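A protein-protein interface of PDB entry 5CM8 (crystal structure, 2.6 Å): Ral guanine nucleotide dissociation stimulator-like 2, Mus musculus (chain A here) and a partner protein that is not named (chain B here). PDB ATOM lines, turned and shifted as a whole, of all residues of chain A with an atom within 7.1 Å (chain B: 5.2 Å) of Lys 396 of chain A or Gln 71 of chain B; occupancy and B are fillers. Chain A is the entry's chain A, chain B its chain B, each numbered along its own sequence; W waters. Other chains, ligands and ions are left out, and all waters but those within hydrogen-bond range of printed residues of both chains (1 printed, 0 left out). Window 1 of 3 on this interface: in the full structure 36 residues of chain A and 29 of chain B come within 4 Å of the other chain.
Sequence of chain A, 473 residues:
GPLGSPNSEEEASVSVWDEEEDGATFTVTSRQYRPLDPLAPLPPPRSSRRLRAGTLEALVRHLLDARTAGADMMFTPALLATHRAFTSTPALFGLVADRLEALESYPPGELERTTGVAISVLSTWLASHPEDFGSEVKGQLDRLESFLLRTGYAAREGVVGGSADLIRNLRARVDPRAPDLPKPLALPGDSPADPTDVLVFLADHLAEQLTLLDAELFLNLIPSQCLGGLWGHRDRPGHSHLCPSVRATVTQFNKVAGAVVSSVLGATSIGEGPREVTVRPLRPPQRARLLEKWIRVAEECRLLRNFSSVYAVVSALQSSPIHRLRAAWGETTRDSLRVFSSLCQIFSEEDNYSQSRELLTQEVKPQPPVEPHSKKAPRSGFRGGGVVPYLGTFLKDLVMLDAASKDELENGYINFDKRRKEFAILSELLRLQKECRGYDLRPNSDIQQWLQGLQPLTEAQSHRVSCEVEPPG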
ATOM      1  N   CYS A 226      10.806  18.486  22.813  1.00  0.00           N
ATOM      2  CA  CYS A 226       9.743  18.091  21.886  1.00  0.00           C
ATOM      3  C   CYS A 226      10.225  17.075  20.851  1.00  0.00           C
ATOM      4  O   CYS A 226       9.416  16.525  20.094  1.00  0.00           O
ATOM      5  CB  CYS A 226       9.162  19.317  21.170  1.00  0.00           C
ATOM      6  SG  CYS A 226       8.511  20.614  22.252  1.00  0.00           S
ATOM      7  N   TRP A 231      10.332  12.864  23.442  1.00  0.00           N
ATOM      8  CA  TRP A 231       8.895  12.900  23.709  1.00  0.00           C
ATOM      9  C   TRP A 231       8.195  11.573  23.404  1.00  0.00           C
ATOM     10  O   TRP A 231       7.257  11.190  24.109  1.00  0.00           O
ATOM     11  CB  TRP A 231       8.232  14.053  22.945  1.00  0.00           C
ATOM     12  CG  TRP A 231       6.736  14.144  23.129  1.00  0.00           C
ATOM     13  CD1 TRP A 231       5.783  13.912  22.183  1.00  0.00           C
ATOM     14  CD2 TRP A 231       6.031  14.486  24.333  1.00  0.00           C
ATOM     15  NE1 TRP A 231       4.529  14.089  22.716  1.00  0.00           N
ATOM     16  CE2 TRP A 231       4.651  14.444  24.034  1.00  0.00           C
ATOM     17  CE3 TRP A 231       6.429  14.830  25.632  1.00  0.00           C
ATOM     18  CZ2 TRP A 231       3.665  14.729  24.988  1.00  0.00           C
ATOM     19  CZ3 TRP A 231       5.449  15.112  26.579  1.00  0.00           C
ATOM     20  CH2 TRP A 231       4.085  15.061  26.251  1.00  0.00           C
ATOM     21  N   ARG A 234       8.259   8.950  26.328  1.00  0.00           N
ATOM     22  CA  ARG A 234       7.789   9.496  27.602  1.00  0.00           C
ATOM     23  C   ARG A 234       7.134   8.450  28.505  1.00  0.00           C
ATOM     24  O   ARG A 234       7.257   8.517  29.731  1.00  0.00           O
ATOM     25  CB  ARG A 234       6.842  10.687  27.365  1.00  0.00           C
ATOM     26  CG  ARG A 234       5.350  10.351  27.295  1.00  0.00           C
ATOM     27  CD  ARG A 234       4.515  11.522  26.789  1.00  0.00           C
ATOM     28  NE  ARG A 234       4.398  11.503  25.333  1.00  0.00           N
ATOM     29  CZ  ARG A 234       3.309  11.144  24.659  1.00  0.00           C
ATOM     30  NH1 ARG A 234       2.202  10.781  25.293  1.00  0.00           N
ATOM     31  NH2 ARG A 234       3.325  11.157  23.339  1.00  0.00           N
ATOM     32  N   VAL A 250       0.544  20.524  27.779  1.00  0.00           N
ATOM     33  CA  VAL A 250      -0.557  19.588  27.574  1.00  0.00           C
ATOM     34  C   VAL A 250      -1.551  19.637  28.748  1.00  0.00           C
ATOM     35  O   VAL A 250      -2.770  19.597  28.545  1.00  0.00           O
ATOM     36  CB  VAL A 250      -0.020  18.145  27.352  1.00  0.00           C
ATOM     37  CG1 VAL A 250      -1.156  17.117  27.290  1.00  0.00           C
ATOM     38  CG2 VAL A 250       0.837  18.082  26.089  1.00  0.00           C
ATOM     39  N   TYR A 311      -8.335  25.604  20.125  1.00  0.00           N
ATOM     40  CA  TYR A 311      -8.467  24.180  19.862  1.00  0.00           C
ATOM     41  C   TYR A 311      -8.905  23.387  21.085  1.00  0.00           C
ATOM     42  O   TYR A 311      -9.574  22.372  20.943  1.00  0.00           O
ATOM     43  CB  TYR A 311      -7.174  23.606  19.278  1.00  0.00           C
ATOM     44  CG  TYR A 311      -7.347  22.243  18.642  1.00  0.00           C
ATOM     45  CD1 TYR A 311      -8.458  21.959  17.845  1.00  0.00           C
ATOM     46  CD2 TYR A 311      -6.398  21.241  18.827  1.00  0.00           C
ATOM     47  CE1 TYR A 311      -8.626  20.708  17.253  1.00  0.00           C
ATOM     48  CE2 TYR A 311      -6.555  19.982  18.236  1.00  0.00           C
ATOM     49  CZ  TYR A 311      -7.673  19.725  17.454  1.00  0.00           C
ATOM     50  OH  TYR A 311      -7.835  18.489  16.864  1.00  0.00           O
ATOM     51  N   GLU A 349      -8.670  18.348  10.727  1.00  0.00           N
ATOM     52  CA  GLU A 349      -7.514  17.525  10.392  1.00  0.00           C
ATOM     53  C   GLU A 349      -7.276  17.491   8.887  1.00  0.00           C
ATOM     54  O   GLU A 349      -6.214  17.061   8.430  1.00  0.00           O
ATOM     55  CB  GLU A 349      -7.708  16.095  10.907  1.00  0.00           C
ATOM     56  CG  GLU A 349      -8.653  15.963  12.096  1.00  0.00           C
ATOM     57  CD  GLU A 349     -10.119  15.930  11.689  1.00  0.00           C
ATOM     58  OE1 GLU A 349     -10.412  15.670  10.500  1.00  0.00           O
ATOM     59  OE2 GLU A 349     -10.980  16.164  12.564  1.00  0.00           O
ATOM     60  N   ASN A 352      -3.801  17.521   6.295  1.00  0.00           N
ATOM     61  CA  ASN A 352      -2.742  17.635   7.307  1.00  0.00           C
ATOM     62  C   ASN A 352      -2.739  18.982   8.046  1.00  0.00           C
ATOM     63  O   ASN A 352      -1.707  19.657   8.128  1.00  0.00           O
ATOM     64  CB  ASN A 352      -1.367  17.320   6.689  1.00  0.00           C
ATOM     65  CG  ASN A 352      -0.261  17.162   7.732  1.00  0.00           C
ATOM     66  OD1 ASN A 352      -0.513  16.842   8.900  1.00  0.00           O
ATOM     67  ND2 ASN A 352       0.977  17.382   7.303  1.00  0.00           N
ATOM     68  N   TYR A 353      -3.911  19.361   8.564  1.00  0.00           N
ATOM     69  CA  TYR A 353      -4.100  20.587   9.354  1.00  0.00           C
ATOM     70  C   TYR A 353      -3.648  21.865   8.645  1.00  0.00           C
ATOM     71  O   TYR A 353      -3.236  22.830   9.297  1.00  0.00           O
ATOM     72  CB  TYR A 353      -3.397  20.485  10.716  1.00  0.00           C
ATOM     73  CG  TYR A 353      -3.853  19.334  11.572  1.00  0.00           C
ATOM     74  CD1 TYR A 353      -3.351  18.051  11.367  1.00  0.00           C
ATOM     75  CD2 TYR A 353      -4.774  19.526  12.597  1.00  0.00           C
ATOM     76  CE1 TYR A 353      -3.761  16.987  12.150  1.00  0.00           C
ATOM     77  CE2 TYR A 353      -5.192  18.464  13.390  1.00  0.00           C
ATOM     78  CZ  TYR A 353      -4.679  17.199  13.157  1.00  0.00           C
ATOM     79  OH  TYR A 353      -5.071  16.137  13.925  1.00  0.00           O
ATOM     80  N   ARG A 357      -2.042  25.192  10.342  1.00  0.00           N
ATOM     81  CA  ARG A 357      -0.617  25.349  10.031  1.00  0.00           C
ATOM     82  C   ARG A 357      -0.327  26.674   9.333  1.00  0.00           C
ATOM     83  O   ARG A 357       0.718  27.285   9.560  1.00  0.00           O
ATOM     84  CB  ARG A 357      -0.124  24.214   9.135  1.00  0.00           C
ATOM     85  CG  ARG A 357       0.026  22.861   9.798  1.00  0.00           C
ATOM     86  CD  ARG A 357       0.697  21.905   8.825  1.00  0.00           C
ATOM     87  NE  ARG A 357       0.786  20.533   9.319  1.00  0.00           N
ATOM     88  CZ  ARG A 357       1.768  20.072  10.087  1.00  0.00           C
ATOM     89  NH1 ARG A 357       2.748  20.873  10.486  1.00  0.00           N
ATOM     90  NH2 ARG A 357       1.761  18.805  10.479  1.00  0.00           N
ATOM     91  N   TYR A 390      -1.029  25.610  18.883  1.00  0.00           N
ATOM     92  CA  TYR A 390      -1.350  24.293  19.409  1.00  0.00           C
ATOM     93  C   TYR A 390      -0.126  23.402  19.202  1.00  0.00           C
ATOM     94  O   TYR A 390       0.302  23.177  18.066  1.00  0.00           O
ATOM     95  CB  TYR A 390      -2.580  23.718  18.706  1.00  0.00           C
ATOM     96  CG  TYR A 390      -2.794  22.246  18.962  1.00  0.00           C
ATOM     97  CD1 TYR A 390      -3.077  21.775  20.244  1.00  0.00           C
ATOM     98  CD2 TYR A 390      -2.705  21.321  17.924  1.00  0.00           C
ATOM     99  CE1 TYR A 390      -3.265  20.422  20.487  1.00  0.00           C
ATOM    100  CE2 TYR A 390      -2.894  19.965  18.157  1.00  0.00           C
ATOM    101  CZ  TYR A 390      -3.173  19.526  19.441  1.00  0.00           C
ATOM    102  OH  TYR A 390      -3.359  18.192  19.681  1.00  0.00           O
ATOM    103  N   LEU A 391       0.439  22.911  20.301  1.00  0.00           N
ATOM    104  CA  LEU A 391       1.733  22.230  20.255  1.00  0.00           C
ATOM    105  C   LEU A 391       1.665  20.843  19.631  1.00  0.00           C
ATOM    106  O   LEU A 391       2.638  20.385  19.025  1.00  0.00           O
ATOM    107  CB  LEU A 391       2.373  22.161  21.649  1.00  0.00           C
ATOM    108  CG  LEU A 391       3.850  21.744  21.681  1.00  0.00           C
ATOM    109  CD1 LEU A 391       4.764  22.791  21.031  1.00  0.00           C
ATOM    110  CD2 LEU A 391       4.310  21.422  23.098  1.00  0.00           C
ATOM    111  N   GLY A 392       0.519  20.183  19.788  1.00  0.00           N
ATOM    112  CA  GLY A 392       0.316  18.817  19.297  1.00  0.00           C
ATOM    113  C   GLY A 392       0.809  18.563  17.886  1.00  0.00           C
ATOM    114  O   GLY A 392       1.520  17.590  17.637  1.00  0.00           O
ATOM    115  N   THR A 393       0.436  19.453  16.970  1.00  0.00           N
ATOM    116  CA  THR A 393       0.853  19.381  15.568  1.00  0.00           C
ATOM    117  C   THR A 393       2.382  19.310  15.426  1.00  0.00           C
ATOM    118  O   THR A 393       2.895  18.540  14.619  1.00  0.00           O
ATOM    119  CB  THR A 393       0.273  20.567  14.758  1.00  0.00           C
ATOM    120  OG1 THR A 393      -1.147  20.627  14.946  1.00  0.00           O
ATOM    121  CG2 THR A 393       0.555  20.417  13.281  1.00  0.00           C
ATOM    122  N   PHE A 394       3.101  20.096  16.225  1.00  0.00           N
ATOM    123  CA  PHE A 394       4.563  20.064  16.234  1.00  0.00           C
ATOM    124  C   PHE A 394       5.088  18.742  16.796  1.00  0.00           C
ATOM    125  O   PHE A 394       6.018  18.149  16.241  1.00  0.00           O
ATOM    126  CB  PHE A 394       5.134  21.258  17.015  1.00  0.00           C
ATOM    127  CG  PHE A 394       4.864  22.587  16.368  1.00  0.00           C
ATOM    128  CD1 PHE A 394       3.679  23.266  16.618  1.00  0.00           C
ATOM    129  CD2 PHE A 394       5.791  23.153  15.502  1.00  0.00           C
ATOM    130  CE1 PHE A 394       3.417  24.491  16.013  1.00  0.00           C
ATOM    131  CE2 PHE A 394       5.543  24.380  14.888  1.00  0.00           C
ATOM    132  CZ  PHE A 394       4.351  25.052  15.145  1.00  0.00           C
ATOM    133  N   LEU A 395       4.485  18.279  17.890  1.00  0.00           N
ATOM    134  CA  LEU A 395       4.856  16.992  18.480  1.00  0.00           C
ATOM    135  C   LEU A 395       4.615  15.818  17.515  1.00  0.00           C
ATOM    136  O   LEU A 395       5.411  14.878  17.460  1.00  0.00           O
ATOM    137  CB  LEU A 395       4.135  16.769  19.814  1.00  0.00           C
ATOM    138  CG  LEU A 395       4.396  17.794  20.926  1.00  0.00           C
ATOM    139  CD1 LEU A 395       3.320  17.707  22.000  1.00  0.00           C
ATOM    140  CD2 LEU A 395       5.790  17.634  21.531  1.00  0.00           C
ATOM    141  N   LYS A 396       3.532  15.886  16.745  1.00  0.00           N
ATOM    142  CA  LYS A 396       3.249  14.866  15.739  1.00  0.00           C
ATOM    143  C   LYS A 396       4.341  14.833  14.671  1.00  0.00           C
ATOM    144  O   LYS A 396       4.827  13.760  14.310  1.00  0.00           O
ATOM    145  CB  LYS A 396       1.875  15.085  15.092  1.00  0.00           C
ATOM    146  CG  LYS A 396       1.394  13.904  14.249  1.00  0.00           C
ATOM    147  CD  LYS A 396       0.172  14.252  13.387  1.00  0.00           C
ATOM    148  CE  LYS A 396       0.557  15.100  12.180  1.00  0.00           C
ATOM    149  NZ  LYS A 396      -0.633  15.694  11.505  1.00  0.00           N
ATOM    150  N   ASP A 397       4.726  16.010  14.182  1.00  0.00           N
ATOM    151  CA  ASP A 397       5.757  16.121  13.157  1.00  0.00           C
ATOM    152  C   ASP A 397       7.079  15.524  13.636  1.00  0.00           C
ATOM    153  O   ASP A 397       7.705  14.738  12.928  1.00  0.00           O
ATOM    154  CB  ASP A 397       5.950  17.586  12.740  1.00  0.00           C
ATOM    155  CG  ASP A 397       4.722  18.175  12.056  1.00  0.00           C
ATOM    156  OD1 ASP A 397       3.855  17.405  11.589  1.00  0.00           O
ATOM    157  OD2 ASP A 397       4.625  19.421  11.982  1.00  0.00           O
ATOM    158  N   LEU A 398       7.481  15.884  14.851  1.00  0.00           N
ATOM    159  CA  LEU A 398       8.764  15.462  15.400  1.00  0.00           C
ATOM    160  C   LEU A 398       8.828  13.972  15.732  1.00  0.00           C
ATOM    161  O   LEU A 398       9.861  13.337  15.513  1.00  0.00           O
ATOM    162  CB  LEU A 398       9.147  16.328  16.607  1.00  0.00           C
ATOM    163  CG  LEU A 398       9.538  17.772  16.264  1.00  0.00           C
ATOM    164  CD1 LEU A 398       9.433  18.692  17.477  1.00  0.00           C
ATOM    165  CD2 LEU A 398      10.934  17.842  15.643  1.00  0.00           C
ATOM    166  N   VAL A 399       7.731  13.421  16.251  1.00  0.00           N
ATOM    167  CA  VAL A 399       7.623  11.976  16.486  1.00  0.00           C
ATOM    168  C   VAL A 399       7.646  11.224  15.161  1.00  0.00           C
ATOM    169  O   VAL A 399       8.316  10.199  15.032  1.00  0.00           O
ATOM    170  CB  VAL A 399       6.353  11.608  17.308  1.00  0.00           C
ATOM    171  CG1 VAL A 399       5.835  10.211  16.969  1.00  0.00           C
ATOM    172  CG2 VAL A 399       6.633  11.716  18.790  1.00  0.00           C
ATOM    173  N   MET A 400       6.917  11.751  14.182  1.00  0.00           N
ATOM    174  CA  MET A 400       6.849  11.163  12.856  1.00  0.00           C
ATOM    175  C   MET A 400       8.221  11.200  12.202  1.00  0.00           C
ATOM    176  O   MET A 400       8.650  10.226  11.571  1.00  0.00           O
ATOM    177  CB  MET A 400       5.843  11.926  11.994  1.00  0.00           C
ATOM    178  CG  MET A 400       5.123  11.071  10.969  1.00  0.00           C
ATOM    179  SD  MET A 400       4.051   9.810  11.689  1.00  0.00           S
ATOM    180  CE  MET A 400       2.717  10.807  12.355  1.00  0.00           C
ATOM    181  N   LEU A 401       8.907  12.328  12.376  1.00  0.00           N
ATOM    182  CA  LEU A 401      10.214  12.563  11.776  1.00  0.00           C
ATOM    183  C   LEU A 401      11.273  11.691  12.438  1.00  0.00           C
ATOM    184  O   LEU A 401      12.221  11.258  11.788  1.00  0.00           O
ATOM    185  CB  LEU A 401      10.577  14.042  11.902  1.00  0.00           C
ATOM    186  CG  LEU A 401      11.320  14.784  10.788  1.00  0.00           C
ATOM    187  CD1 LEU A 401      10.742  14.530   9.403  1.00  0.00           C
ATOM    188  CD2 LEU A 401      11.277  16.259  11.095  1.00  0.00           C
ATOM    189  N   ASP A 402      11.092  11.425  13.730  1.00  0.00           N
ATOM    190  CA  ASP A 402      11.978  10.536  14.481  1.00  0.00           C
ATOM    191  C   ASP A 402      11.958   9.100  13.951  1.00  0.00           C
ATOM    192  O   ASP A 402      12.971   8.404  13.998  1.00  0.00           O
ATOM    193  CB  ASP A 402      11.609  10.541  15.964  1.00  0.00           C
ATOM    194  CG  ASP A 402      12.559   9.712  16.809  1.00  0.00           C
ATOM    195  OD1 ASP A 402      13.787   9.896  16.679  1.00  0.00           O
ATOM    196  OD2 ASP A 402      12.078   8.874  17.604  1.00  0.00           O
ATOM    197  N   TYR B  50      -0.386  12.748   4.393  1.00  0.00           N
ATOM    198  CA  TYR B  50      -1.059  11.519   4.813  1.00  0.00           C
ATOM    199  C   TYR B  50      -2.131  11.043   3.830  1.00  0.00           C
ATOM    200  O   TYR B  50      -3.090  10.371   4.219  1.00  0.00           O
ATOM    201  CB  TYR B  50      -1.628  11.678   6.227  1.00  0.00           C
ATOM    202  CG  TYR B  50      -0.586  12.043   7.258  1.00  0.00           C
ATOM    203  CD1 TYR B  50      -0.517  13.332   7.776  1.00  0.00           C
ATOM    204  CD2 TYR B  50       0.343  11.104   7.704  1.00  0.00           C
ATOM    205  CE1 TYR B  50       0.442  13.676   8.717  1.00  0.00           C
ATOM    206  CE2 TYR B  50       1.308  11.439   8.645  1.00  0.00           C
ATOM    207  CZ  TYR B  50       1.351  12.726   9.146  1.00  0.00           C
ATOM    208  OH  TYR B  50       2.301  13.066  10.078  1.00  0.00           O
ATOM    209  N   ASP B  67      -3.257   9.940  12.292  1.00  0.00           N
ATOM    210  CA  ASP B  67      -2.522   9.322  13.386  1.00  0.00           C
ATOM    211  C   ASP B  67      -2.380  10.294  14.549  1.00  0.00           C
ATOM    212  O   ASP B  67      -2.001  11.453  14.358  1.00  0.00           O
ATOM    213  CB  ASP B  67      -1.143   8.850  12.904  1.00  0.00           C
ATOM    214  CG  ASP B  67      -0.439   7.941  13.910  1.00  0.00           C
ATOM    215  OD1 ASP B  67      -0.981   7.701  15.016  1.00  0.00           O
ATOM    216  OD2 ASP B  67       0.673   7.463  13.590  1.00  0.00           O
ATOM    217  N   THR B  68      -2.686   9.802  15.747  1.00  0.00           N
ATOM    218  CA  THR B  68      -2.604  10.585  16.985  1.00  0.00           C
ATOM    219  C   THR B  68      -1.187  10.611  17.573  1.00  0.00           C
ATOM    220  O   THR B  68      -1.003  10.936  18.749  1.00  0.00           O
ATOM    221  CB  THR B  68      -3.568  10.035  18.061  1.00  0.00           C
ATOM    222  OG1 THR B  68      -3.336   8.633  18.244  1.00  0.00           O
ATOM    223  CG2 THR B  68      -5.014  10.258  17.659  1.00  0.00           C
ATOM    224  N   ALA B  69      -0.198  10.269  16.750  1.00  0.00           N
ATOM    225  CA  ALA B  69       1.203  10.211  17.170  1.00  0.00           C
ATOM    226  C   ALA B  69       1.634  11.468  17.926  1.00  0.00           C
ATOM    227  O   ALA B  69       1.511  12.583  17.415  1.00  0.00           O
ATOM    228  CB  ALA B  69       2.106   9.975  15.964  1.00  0.00           C
ATOM    229  N   GLY B  70       2.117  11.275  19.150  1.00  0.00           N
ATOM    230  CA  GLY B  70       2.564  12.376  20.001  1.00  0.00           C
ATOM    231  C   GLY B  70       1.445  13.104  20.728  1.00  0.00           C
ATOM    232  O   GLY B  70       1.696  13.820  21.702  1.00  0.00           O
ATOM    233  N   GLN B  71       0.210  12.908  20.267  1.00  0.00           N
ATOM    234  CA  GLN B  71      -0.943  13.653  20.767  1.00  0.00           C
ATOM    235  C   GLN B  71      -1.849  12.819  21.678  1.00  0.00           C
ATOM    236  O   GLN B  71      -3.031  13.136  21.846  1.00  0.00           O
ATOM    237  CB  GLN B  71      -1.750  14.207  19.590  1.00  0.00           C
ATOM    238  CG  GLN B  71      -0.931  15.027  18.601  1.00  0.00           C
ATOM    239  CD  GLN B  71      -1.743  15.493  17.411  1.00  0.00           C
ATOM    240  OE1 GLN B  71      -2.538  16.427  17.514  1.00  0.00           O
ATOM    241  NE2 GLN B  71      -1.541  14.846  16.268  1.00  0.00           N
ATOM    242  N   GLU B  72      -1.286  11.775  22.281  1.00  0.00           N
ATOM    243  CA  GLU B  72      -2.066  10.793  23.043  1.00  0.00           C
ATOM    244  C   GLU B  72      -2.515  11.295  24.415  1.00  0.00           C
ATOM    245  O   GLU B  72      -3.436  10.734  25.010  1.00  0.00           O
ATOM    246  CB  GLU B  72      -1.294   9.472  23.207  1.00  0.00           C
ATOM    247  CG  GLU B  72      -0.785   8.840  21.908  1.00  0.00           C
ATOM    248  CD  GLU B  72       0.612   9.311  21.521  1.00  0.00           C
ATOM    249  OE1 GLU B  72       1.139  10.246  22.162  1.00  0.00           O
ATOM    250  OE2 GLU B  72       1.187   8.739  20.574  1.00  0.00           O
ATOM    251  N   ASP B  73      -1.869  12.343  24.916  1.00  0.00           N
ATOM    252  CA  ASP B  73      -2.183  12.863  26.246  1.00  0.00           C
ATOM    253  C   ASP B  73      -3.266  13.951  26.219  1.00  0.00           C
ATOM    254  O   ASP B  73      -3.798  14.318  27.264  1.00  0.00           O
ATOM    255  CB  ASP B  73      -0.912  13.361  26.951  1.00  0.00           C
ATOM    256  CG  ASP B  73       0.150  12.269  27.105  1.00  0.00           C
ATOM    257  OD1 ASP B  73      -0.164  11.073  26.923  1.00  0.00           O
ATOM    258  OD2 ASP B  73       1.314  12.604  27.411  1.00  0.00           O
ATOM    259  N   TYR B  74      -3.596  14.448  25.027  1.00  0.00           N
ATOM    260  CA  TYR B  74      -4.641  15.469  24.879  1.00  0.00           C
ATOM    261  C   TYR B  74      -6.042  14.923  25.155  1.00  0.00           C
ATOM    262  O   TYR B  74      -6.372  13.807  24.754  1.00  0.00           O
ATOM    263  CB  TYR B  74      -4.582  16.124  23.495  1.00  0.00           C
ATOM    264  CG  TYR B  74      -3.371  16.999  23.279  1.00  0.00           C
ATOM    265  CD1 TYR B  74      -2.359  16.610  22.408  1.00  0.00           C
ATOM    266  CD2 TYR B  74      -3.233  18.216  23.949  1.00  0.00           C
ATOM    267  CE1 TYR B  74      -1.241  17.407  22.205  1.00  0.00           C
ATOM    268  CE2 TYR B  74      -2.116  19.024  23.756  1.00  0.00           C
ATOM    269  CZ  TYR B  74      -1.124  18.611  22.881  1.00  0.00           C
ATOM    270  OH  TYR B  74      -0.016  19.395  22.675  1.00  0.00           O
ATOM    271  N   ILE B  77      -9.517  15.871  21.865  1.00  0.00           N
ATOM    272  CA  ILE B  77      -9.270  15.929  20.420  1.00  0.00           C
ATOM    273  C   ILE B  77      -9.644  14.665  19.639  1.00  0.00           C
ATOM    274  O   ILE B  77     -10.075  14.761  18.494  1.00  0.00           O
ATOM    275  CB  ILE B  77      -7.813  16.389  20.078  1.00  0.00           C
ATOM    276  CG1 ILE B  77      -6.776  15.338  20.494  1.00  0.00           C
ATOM    277  CG2 ILE B  77      -7.512  17.732  20.731  1.00  0.00           C
ATOM    278  CD1 ILE B  77      -5.427  15.493  19.808  1.00  0.00           C
ATOM    279  N   ARG B  78      -9.501  13.494  20.257  1.00  0.00           N
ATOM    280  CA  ARG B  78      -9.759  12.233  19.558  1.00  0.00           C
ATOM    281  C   ARG B  78     -11.235  12.004  19.240  1.00  0.00           C
ATOM    282  O   ARG B  78     -11.560  11.380  18.230  1.00  0.00           O
ATOM    283  CB  ARG B  78      -9.175  11.039  20.317  1.00  0.00           C
ATOM    284  CG  ARG B  78      -9.882  10.667  21.621  1.00  0.00           C
ATOM    285  CD  ARG B  78      -8.967   9.805  22.470  1.00  0.00           C
ATOM    286  NE  ARG B  78      -7.774  10.558  22.850  1.00  0.00           N
ATOM    287  CZ  ARG B  78      -6.544  10.059  22.915  1.00  0.00           C
ATOM    288  NH1 ARG B  78      -6.313   8.783  22.621  1.00  0.00           N
ATOM    289  NH2 ARG B  78      -5.538  10.851  23.269  1.00  0.00           N
ATOM    290  N   TYR B  81     -11.732  13.094  15.939  1.00  0.00           N
ATOM    291  CA  TYR B  81     -10.982  12.260  15.001  1.00  0.00           C
ATOM    292  C   TYR B  81     -11.832  11.041  14.650  1.00  0.00           C
ATOM    293  O   TYR B  81     -12.012  10.719  13.472  1.00  0.00           O
ATOM    294  CB  TYR B  81      -9.640  11.818  15.601  1.00  0.00           C
ATOM    295  CG  TYR B  81      -8.586  12.907  15.758  1.00  0.00           C
ATOM    296  CD1 TYR B  81      -8.933  14.258  15.814  1.00  0.00           C
ATOM    297  CD2 TYR B  81      -7.237  12.574  15.882  1.00  0.00           C
ATOM    298  CE1 TYR B  81      -7.969  15.247  15.973  1.00  0.00           C
ATOM    299  CE2 TYR B  81      -6.262  13.556  16.040  1.00  0.00           C
ATOM    300  CZ  TYR B  81      -6.637  14.888  16.087  1.00  0.00           C
ATOM    301  OH  TYR B  81      -5.678  15.868  16.241  1.00  0.00           O
HETATM  302  O   HOH W   1       2.019  10.322  28.735  1.00  0.00           O
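OH of Tyr 311 of chain A lies close to OH of Tyr 81 of chain B (3.5 Å).
The backbone NH (N) of Gly 392 of chain A is in hydrogen-bond range of the side-chain hydroxyl (OH) of Tyr 74 of chain B (3.0 Å).
The side-chain carboxylate (OD1) of Asp 73 of chain B lies within salt-bridge range of the guanidinium group (NH1) of Arg 234 of chain A (2.9 Å).
The side-chain hydroxyl (OH) of Tyr 353 of chain A is in hydrogen-bond range of the side-chain hydroxyl (OH) of Tyr 81 of chain B (2.4 Å).
O of Gly 70 of chain B is in hydrogen-bond range of NE1 of Trp 231 of chain A, at 3.0 Å.
The guanidinium group of Arg 234 of chain A lies within salt-bridge range of the side-chain carboxylate of Glu 72 of chain B (2.6 Å).
OH of Tyr 390 of chain A is in hydrogen-bond range of OE1 of Gln 71 of chain B, 2.9 Å away.
OE1 of Gln 71 of chain B sits at hydrogen-bond distance from OH of Tyr 81 of chain B, 3.4 Å away.
NH2 of Arg 78 of chain B lies within hydrogen-bond range of O of Tyr 74 of chain B, 3.4 Å away.
Printed residues of chain B within 4 Å of Leu 391 of chain A: Tyr 74 (3.8 Å).
Phe 394 of chain A touches none of the printed residues of chain B.
Of chain A, only Tyr 390, Gly 392 and Lys 396 come within 4 Å of Gln 71 of chain B.
Of the printed residues of chain A, Glu 72 of chain B touches Arg 234 (2.6 Å).
The nearest residue of chain B that does not touch Lys 396 of chain A is Gly 70 of chain B (4.9 Å).
The nearest residue of chain A that does not touch Gln 71 of chain B is Thr 393 of chain A (4.3 Å).
Of the 12 printed residues of chain B, 10 touch a printed residue of chain A.
Hydrophobic or aromatic side chains of chain B within 4 Å of the printed part of chain A: Tyr 50, Ala 69, Tyr 74, Ile 77 and Tyr 81.
Among the printed residues, Asp or Glu carboxylates within 4 Å of a Lys or Arg side-chain nitrogen of the other chain: Arg 234 of chain A with Glu 72 of chain B and Arg 234 of chain A with Asp 73 of chain B.
Water W1 lies within hydrogen-bond range of OD2 of Asp 73 of chain B (2.7 Å) and NH1 of Arg 234 of chain A (3.5 Å).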
